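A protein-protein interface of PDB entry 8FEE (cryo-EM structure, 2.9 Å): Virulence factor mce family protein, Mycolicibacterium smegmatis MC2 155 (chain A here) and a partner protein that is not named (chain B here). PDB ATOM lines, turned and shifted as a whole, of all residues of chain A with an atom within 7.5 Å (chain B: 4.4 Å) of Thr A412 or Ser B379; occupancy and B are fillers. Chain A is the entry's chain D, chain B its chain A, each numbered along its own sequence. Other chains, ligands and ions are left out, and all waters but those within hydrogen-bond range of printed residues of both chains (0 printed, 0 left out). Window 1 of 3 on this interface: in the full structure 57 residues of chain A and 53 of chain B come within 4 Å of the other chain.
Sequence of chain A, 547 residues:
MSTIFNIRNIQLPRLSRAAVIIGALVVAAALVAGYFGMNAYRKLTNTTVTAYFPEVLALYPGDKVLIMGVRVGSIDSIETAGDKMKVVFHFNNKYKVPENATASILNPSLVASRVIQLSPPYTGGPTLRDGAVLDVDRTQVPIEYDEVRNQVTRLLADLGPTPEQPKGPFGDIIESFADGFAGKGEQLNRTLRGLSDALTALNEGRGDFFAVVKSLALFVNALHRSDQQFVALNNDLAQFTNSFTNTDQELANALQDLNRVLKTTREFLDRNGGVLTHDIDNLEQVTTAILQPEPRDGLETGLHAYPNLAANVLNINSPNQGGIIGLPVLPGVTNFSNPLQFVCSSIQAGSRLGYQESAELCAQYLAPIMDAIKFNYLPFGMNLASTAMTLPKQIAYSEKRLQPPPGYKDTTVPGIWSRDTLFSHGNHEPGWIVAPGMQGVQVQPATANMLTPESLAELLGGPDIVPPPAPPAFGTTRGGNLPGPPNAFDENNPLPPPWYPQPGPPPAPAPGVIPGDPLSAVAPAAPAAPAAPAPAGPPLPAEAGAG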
ATOM      1  N   ASN A 315      26.709  -0.327   9.163  1.00  0.00           N
ATOM      2  CA  ASN A 315      25.951   0.849   8.751  1.00  0.00           C
ATOM      3  C   ASN A 315      25.096   1.435   9.867  1.00  0.00           C
ATOM      4  O   ASN A 315      24.740   2.615   9.798  1.00  0.00           O
ATOM      5  CB  ASN A 315      25.058   0.515   7.556  1.00  0.00           C
ATOM      6  CG  ASN A 315      25.811   0.545   6.246  1.00  0.00           C
ATOM      7  OD1 ASN A 315      26.911   1.093   6.161  1.00  0.00           O
ATOM      8  ND2 ASN A 315      25.224  -0.045   5.214  1.00  0.00           N
ATOM      9  N   MET A 389      24.540  12.050  11.162  1.00  0.00           N
ATOM     10  CA  MET A 389      25.208  10.879  11.720  1.00  0.00           C
ATOM     11  C   MET A 389      26.727  11.004  11.677  1.00  0.00           C
ATOM     12  O   MET A 389      27.409  10.580  12.614  1.00  0.00           O
ATOM     13  CB  MET A 389      24.763   9.613  10.990  1.00  0.00           C
ATOM     14  CG  MET A 389      23.277   9.335  11.076  1.00  0.00           C
ATOM     15  SD  MET A 389      22.862   7.701  10.449  1.00  0.00           S
ATOM     16  CE  MET A 389      21.075   7.791  10.447  1.00  0.00           C
ATOM     17  N   ILE A 395      34.810  10.579   7.418  1.00  0.00           N
ATOM     18  CA  ILE A 395      34.612   9.525   6.428  1.00  0.00           C
ATOM     19  C   ILE A 395      35.965   9.077   5.895  1.00  0.00           C
ATOM     20  O   ILE A 395      36.791   9.902   5.487  1.00  0.00           O
ATOM     21  CB  ILE A 395      33.704  10.010   5.289  1.00  0.00           C
ATOM     22  CG1 ILE A 395      32.468  10.708   5.855  1.00  0.00           C
ATOM     23  CG2 ILE A 395      33.296   8.844   4.408  1.00  0.00           C
ATOM     24  CD1 ILE A 395      31.477   9.769   6.493  1.00  0.00           C
ATOM     25  N   LYS A 409      30.528  14.687  -3.977  1.00  0.00           N
ATOM     26  CA  LYS A 409      30.308  14.157  -2.640  1.00  0.00           C
ATOM     27  C   LYS A 409      29.655  12.783  -2.720  1.00  0.00           C
ATOM     28  O   LYS A 409      28.926  12.475  -3.667  1.00  0.00           O
ATOM     29  CB  LYS A 409      29.437  15.102  -1.803  1.00  0.00           C
ATOM     30  CG  LYS A 409      28.032  15.298  -2.347  1.00  0.00           C
ATOM     31  CD  LYS A 409      27.227  16.248  -1.480  1.00  0.00           C
ATOM     32  CE  LYS A 409      25.766  16.262  -1.898  1.00  0.00           C
ATOM     33  NZ  LYS A 409      24.963  17.215  -1.085  1.00  0.00           N
ATOM     34  N   ASP A 410      29.926  11.959  -1.711  1.00  0.00           N
ATOM     35  CA  ASP A 410      29.429  10.591  -1.686  1.00  0.00           C
ATOM     36  C   ASP A 410      27.928  10.575  -1.401  1.00  0.00           C
ATOM     37  O   ASP A 410      27.362  11.528  -0.859  1.00  0.00           O
ATOM     38  CB  ASP A 410      30.186   9.771  -0.639  1.00  0.00           C
ATOM     39  CG  ASP A 410      29.902   8.284  -0.741  1.00  0.00           C
ATOM     40  OD1 ASP A 410      30.225   7.687  -1.788  1.00  0.00           O
ATOM     41  OD2 ASP A 410      29.356   7.713   0.222  1.00  0.00           O
ATOM     42  N   THR A 411      27.282   9.477  -1.776  1.00  0.00           N
ATOM     43  CA  THR A 411      25.853   9.288  -1.556  1.00  0.00           C
ATOM     44  C   THR A 411      25.608   7.996  -0.782  1.00  0.00           C
ATOM     45  O   THR A 411      26.538   7.267  -0.430  1.00  0.00           O
ATOM     46  CB  THR A 411      25.096   9.264  -2.886  1.00  0.00           C
ATOM     47  OG1 THR A 411      25.800   8.440  -3.822  1.00  0.00           O
ATOM     48  CG2 THR A 411      24.970  10.660  -3.449  1.00  0.00           C
ATOM     49  N   THR A 412      24.331   7.715  -0.520  1.00  0.00           N
ATOM     50  CA  THR A 412      23.944   6.573   0.299  1.00  0.00           C
ATOM     51  C   THR A 412      23.979   5.254  -0.460  1.00  0.00           C
ATOM     52  O   THR A 412      23.659   4.215   0.126  1.00  0.00           O
ATOM     53  CB  THR A 412      22.549   6.785   0.889  1.00  0.00           C
ATOM     54  OG1 THR A 412      21.557   6.527  -0.111  1.00  0.00           O
ATOM     55  CG2 THR A 412      22.396   8.207   1.407  1.00  0.00           C
ATOM     56  N   VAL A 413      24.328   5.268  -1.740  1.00  0.00           N
ATOM     57  CA  VAL A 413      24.749   4.080  -2.473  1.00  0.00           C
ATOM     58  C   VAL A 413      26.238   4.240  -2.773  1.00  0.00           C
ATOM     59  O   VAL A 413      26.618   5.162  -3.511  1.00  0.00           O
ATOM     60  CB  VAL A 413      23.939   3.885  -3.760  1.00  0.00           C
ATOM     61  CG1 VAL A 413      24.522   2.751  -4.580  1.00  0.00           C
ATOM     62  CG2 VAL A 413      22.482   3.616  -3.429  1.00  0.00           C
ATOM     63  N   PRO A 414      27.111   3.405  -2.208  1.00  0.00           N
ATOM     64  CA  PRO A 414      28.554   3.648  -2.333  1.00  0.00           C
ATOM     65  C   PRO A 414      29.005   3.613  -3.786  1.00  0.00           C
ATOM     66  O   PRO A 414      28.539   2.797  -4.582  1.00  0.00           O
ATOM     67  CB  PRO A 414      29.180   2.509  -1.520  1.00  0.00           C
ATOM     68  CG  PRO A 414      28.062   1.950  -0.691  1.00  0.00           C
ATOM     69  CD  PRO A 414      26.827   2.153  -1.495  1.00  0.00           C
ATOM     70  N   GLY A 415      29.921   4.517  -4.123  1.00  0.00           N
ATOM     71  CA  GLY A 415      30.481   4.594  -5.450  1.00  0.00           C
ATOM     72  C   GLY A 415      29.767   5.544  -6.387  1.00  0.00           C
ATOM     73  O   GLY A 415      30.354   5.956  -7.393  1.00  0.00           O
ATOM     74  N   ILE A 416      28.527   5.909  -6.088  1.00  0.00           N
ATOM     75  CA  ILE A 416      27.802   6.910  -6.859  1.00  0.00           C
ATOM     76  C   ILE A 416      28.080   8.272  -6.239  1.00  0.00           C
ATOM     77  O   ILE A 416      27.739   8.516  -5.077  1.00  0.00           O
ATOM     78  CB  ILE A 416      26.296   6.612  -6.888  1.00  0.00           C
ATOM     79  CG1 ILE A 416      26.023   5.325  -7.668  1.00  0.00           C
ATOM     80  CG2 ILE A 416      25.536   7.780  -7.494  1.00  0.00           C
ATOM     81  CD1 ILE A 416      24.558   4.971  -7.771  1.00  0.00           C
ATOM     82  N   SER A 418      27.685  12.437  -6.290  1.00  0.00           N
ATOM     83  CA  SER A 418      26.806  13.512  -6.725  1.00  0.00           C
ATOM     84  C   SER A 418      27.538  14.844  -6.652  1.00  0.00           C
ATOM     85  O   SER A 418      28.663  14.935  -6.158  1.00  0.00           O
ATOM     86  CB  SER A 418      25.532  13.550  -5.875  1.00  0.00           C
ATOM     87  OG  SER A 418      25.831  13.816  -4.516  1.00  0.00           O
ATOM     88  N   ASN B 342      19.418   0.431  -3.505  1.00  0.00           N
ATOM     89  CA  ASN B 342      19.974  -0.117  -2.266  1.00  0.00           C
ATOM     90  C   ASN B 342      19.852  -1.633  -2.203  1.00  0.00           C
ATOM     91  O   ASN B 342      19.430  -2.188  -1.194  1.00  0.00           O
ATOM     92  CB  ASN B 342      19.303   0.530  -1.061  1.00  0.00           C
ATOM     93  CG  ASN B 342      19.874   1.896  -0.739  1.00  0.00           C
ATOM     94  OD1 ASN B 342      19.141   2.879  -0.639  1.00  0.00           O
ATOM     95  ND2 ASN B 342      21.188   1.963  -0.570  1.00  0.00           N
ATOM     96  N   TYR B 371      34.667   6.575   9.848  1.00  0.00           N
ATOM     97  CA  TYR B 371      33.729   5.714   9.138  1.00  0.00           C
ATOM     98  C   TYR B 371      34.376   5.135   7.886  1.00  0.00           C
ATOM     99  O   TYR B 371      35.147   5.809   7.198  1.00  0.00           O
ATOM    100  CB  TYR B 371      32.466   6.493   8.779  1.00  0.00           C
ATOM    101  CG  TYR B 371      31.351   5.631   8.245  1.00  0.00           C
ATOM    102  CD1 TYR B 371      30.435   5.048   9.104  1.00  0.00           C
ATOM    103  CD2 TYR B 371      31.206   5.407   6.885  1.00  0.00           C
ATOM    104  CE1 TYR B 371      29.412   4.257   8.627  1.00  0.00           C
ATOM    105  CE2 TYR B 371      30.184   4.617   6.399  1.00  0.00           C
ATOM    106  CZ  TYR B 371      29.289   4.046   7.272  1.00  0.00           C
ATOM    107  OH  TYR B 371      28.268   3.258   6.792  1.00  0.00           O
ATOM    108  N   VAL B 373      33.597   3.251   4.223  1.00  0.00           N
ATOM    109  CA  VAL B 373      32.620   2.973   3.177  1.00  0.00           C
ATOM    110  C   VAL B 373      33.164   1.875   2.273  1.00  0.00           C
ATOM    111  O   VAL B 373      34.337   1.903   1.878  1.00  0.00           O
ATOM    112  CB  VAL B 373      32.274   4.245   2.378  1.00  0.00           C
ATOM    113  CG1 VAL B 373      31.599   5.262   3.272  1.00  0.00           C
ATOM    114  CG2 VAL B 373      33.521   4.865   1.770  1.00  0.00           C
ATOM    115  N   GLY B 377      26.111  -1.264  -1.281  1.00  0.00           N
ATOM    116  CA  GLY B 377      24.773  -0.874  -1.663  1.00  0.00           C
ATOM    117  C   GLY B 377      24.067  -0.009  -0.644  1.00  0.00           C
ATOM    118  O   GLY B 377      22.888   0.310  -0.836  1.00  0.00           O
ATOM    119  N   ALA B 378      24.750   0.377   0.432  1.00  0.00           N
ATOM    120  CA  ALA B 378      24.190   1.260   1.441  1.00  0.00           C
ATOM    121  C   ALA B 378      25.324   1.991   2.141  1.00  0.00           C
ATOM    122  O   ALA B 378      26.427   1.459   2.292  1.00  0.00           O
ATOM    123  CB  ALA B 378      23.348   0.488   2.460  1.00  0.00           C
ATOM    124  N   SER B 379      25.041   3.220   2.567  1.00  0.00           N
ATOM    125  CA  SER B 379      26.034   4.051   3.227  1.00  0.00           C
ATOM    126  C   SER B 379      25.316   5.126   4.029  1.00  0.00           C
ATOM    127  O   SER B 379      24.131   5.392   3.821  1.00  0.00           O
ATOM    128  CB  SER B 379      27.001   4.682   2.219  1.00  0.00           C
ATOM    129  OG  SER B 379      28.098   5.293   2.873  1.00  0.00           O
ATOM    130  N   ILE B 380      26.054   5.733   4.959  1.00  0.00           N
ATOM    131  CA  ILE B 380      25.550   6.865   5.729  1.00  0.00           C
ATOM    132  C   ILE B 380      26.604   7.963   5.712  1.00  0.00           C
ATOM    133  O   ILE B 380      26.663   8.805   6.616  1.00  0.00           O
ATOM    134  CB  ILE B 380      25.186   6.467   7.172  1.00  0.00           C
ATOM    135  CG1 ILE B 380      26.394   5.860   7.883  1.00  0.00           C
ATOM    136  CG2 ILE B 380      24.006   5.504   7.189  1.00  0.00           C
ATOM    137  CD1 ILE B 380      26.123   5.489   9.319  1.00  0.00           C
ATOM    138  N   ALA B 381      27.441   7.955   4.675  1.00  0.00           N
ATOM    139  CA  ALA B 381      28.444   9.003   4.507  1.00  0.00           C
ATOM    140  C   ALA B 381      27.885  10.419   4.352  1.00  0.00           C
ATOM    141  O   ALA B 381      28.445  11.332   4.984  1.00  0.00           O
ATOM    142  CB  ALA B 381      29.345   8.658   3.317  1.00  0.00           C
ATOM    143  N   PRO B 382      26.839  10.695   3.556  1.00  0.00           N
ATOM    144  CA  PRO B 382      26.500  12.100   3.290  1.00  0.00           C
ATOM    145  C   PRO B 382      25.774  12.799   4.428  1.00  0.00           C
ATOM    146  O   PRO B 382      25.584  14.020   4.352  1.00  0.00           O
ATOM    147  CB  PRO B 382      25.614  12.022   2.034  1.00  0.00           C
ATOM    148  CG  PRO B 382      25.239  10.589   1.874  1.00  0.00           C
ATOM    149  CD  PRO B 382      25.781   9.818   3.023  1.00  0.00           C
ATOM    150  N   TYR B 383      25.367  12.078   5.473  1.00  0.00           N
ATOM    151  CA  TYR B 383      24.608  12.679   6.562  1.00  0.00           C
ATOM    152  C   TYR B 383      25.507  13.583   7.397  1.00  0.00           C
ATOM    153  O   TYR B 383      25.821  13.267   8.548  1.00  0.00           O
ATOM    154  CB  TYR B 383      23.988  11.598   7.450  1.00  0.00           C
ATOM    155  CG  TYR B 383      22.814  10.865   6.843  1.00  0.00           C
ATOM    156  CD1 TYR B 383      21.532  11.392   6.910  1.00  0.00           C
ATOM    157  CD2 TYR B 383      22.984   9.634   6.226  1.00  0.00           C
ATOM    158  CE1 TYR B 383      20.453  10.720   6.365  1.00  0.00           C
ATOM    159  CE2 TYR B 383      21.910   8.954   5.680  1.00  0.00           C
ATOM    160  CZ  TYR B 383      20.648   9.501   5.753  1.00  0.00           C
ATOM    161  OH  TYR B 383      19.577   8.830   5.211  1.00  0.00           O
ATOM    162  N   ILE B 407      18.891   8.816  -3.046  1.00  0.00           N
ATOM    163  CA  ILE B 407      20.160   8.384  -2.480  1.00  0.00           C
ATOM    164  C   ILE B 407      21.068   9.558  -2.164  1.00  0.00           C
ATOM    165  O   ILE B 407      22.170   9.359  -1.637  1.00  0.00           O
ATOM    166  CB  ILE B 407      20.875   7.397  -3.423  1.00  0.00           C
ATOM    167  CG1 ILE B 407      21.580   8.149  -4.552  1.00  0.00           C
ATOM    168  CG2 ILE B 407      19.883   6.402  -3.987  1.00  0.00           C
ATOM    169  CD1 ILE B 407      22.186   7.247  -5.593  1.00  0.00           C
ATOM    170  N   PRO B 409      20.332  12.655  -0.038  1.00  0.00           N
ATOM    171  CA  PRO B 409      19.413  13.409   0.816  1.00  0.00           C
ATOM    172  C   PRO B 409      20.023  14.696   1.348  1.00  0.00           C
ATOM    173  O   PRO B 409      21.240  14.878   1.335  1.00  0.00           O
ATOM    174  CB  PRO B 409      19.139  12.435   1.957  1.00  0.00           C
ATOM    175  CG  PRO B 409      20.427  11.701   2.103  1.00  0.00           C
ATOM    176  CD  PRO B 409      21.015  11.587   0.714  1.00  0.00           C
ATOM    177  OXT PRO B 409      19.305  15.580   1.807  1.00  0.00           O
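Printed residues of chain A that touch a printed residue of chain B: Asn A315, Met A389, Ile A395, Asp A410, Thr A411, Thr A412, Val A413, Pro A414 and Ile A416. Hydrophobic or aromatic side chains of chain A within 4 Å of the printed part of chain B: Ile A395, Val A413, Pro A414 and Ile A416. Among the printed residues, no Asp or Glu carboxylate lies within 4 Å of a Lys or Arg side-chain nitrogen of the other chain.
Of chain B, only Asn B342, Ala B378, Ser B379, Pro B382, Ile B407 and Pro B409 come within 4 Å of Thr A412. Of chain A, only Asp A410 (3.8 Å), Thr A411 (3.7 Å) and Thr A412 (3.0 Å) come within 4 Å of Ser B379. Printed residues of chain A within 4 Å of Ile B380: Asn A315 (3.2 Å). Printed residues of chain B within 4 Å of Asp A410: Ser B379, Ala B381 and Pro B382. Of the printed residues of chain B, Asn A315 touches Tyr B371, Ala B378 and Ile B380. Printed residues of chain A within 4 Å of Ile B407: Thr A411, Thr A412, Val A413 and Ile A416. Printed residues of chain B within 4 Å of Pro A414: Gly B377 and Ala B378. Ser A418 touches none of the printed residues of chain B.
Ile A395 touches Tyr B371. Ala B381 touches Ile A395 (CA to CD1, 3.7 Å). Ala B381 touches Asp A410 (CB to OD2, 3.2 Å). CB of Pro B382 touches O of Asp A410, 3.4 Å away. O of Thr A411 touches CB of Ser B379 (3.7 Å). CB of Thr A411 touches O of Ile B407 (3.2 Å). O of Thr A412 touches CA of Ala B378, at 3.3 Å. CG2 of Val A413 touches ND2 of Asn B342 (3.5 Å). Ile B407 touches Val A413 (CG2 to CG2, 3.9 Å). Pro A414 touches Gly B377 (CD to N, 3.5 Å).
ND2 of Asn B342 sits at hydrogen-bond distance from O of Thr A412. The side-chain amide oxygen (OD1) of Asn A315 sits at hydrogen-bond distance from the side-chain hydroxyl (OH) of Tyr B371, at 2.6 Å. The backbone carbonyl oxygen (O) of Ala B378 sits close to the side-chain amide nitrogen (ND2) of Asn A315 (3.5 Å). The backbone NH of Ser B379 lies within hydrogen-bond range of the backbone carbonyl oxygen of Thr A412 (3.0 Å). The backbone carbonyl oxygen (O) of Tyr B383 lies within hydrogen-bond range of the backbone NH (N) of Met A389, at 3.2 Å. The backbone NH of Thr A412 sits at hydrogen-bond distance from the backbone carbonyl oxygen of Ile B407 (2.9 Å).
The side-chain hydroxyl (OG) of Ser B379 sits at hydrogen-bond distance from the backbone NH (N) of Ala B381 (3.3 Å). O of Val A413 lies within hydrogen-bond range of OG1 of Thr A411 (3.4 Å). The backbone NH (N) of Thr A411 lies within hydrogen-bond range of the backbone carbonyl oxygen (O) of Ile A416, 3.5 Å away.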
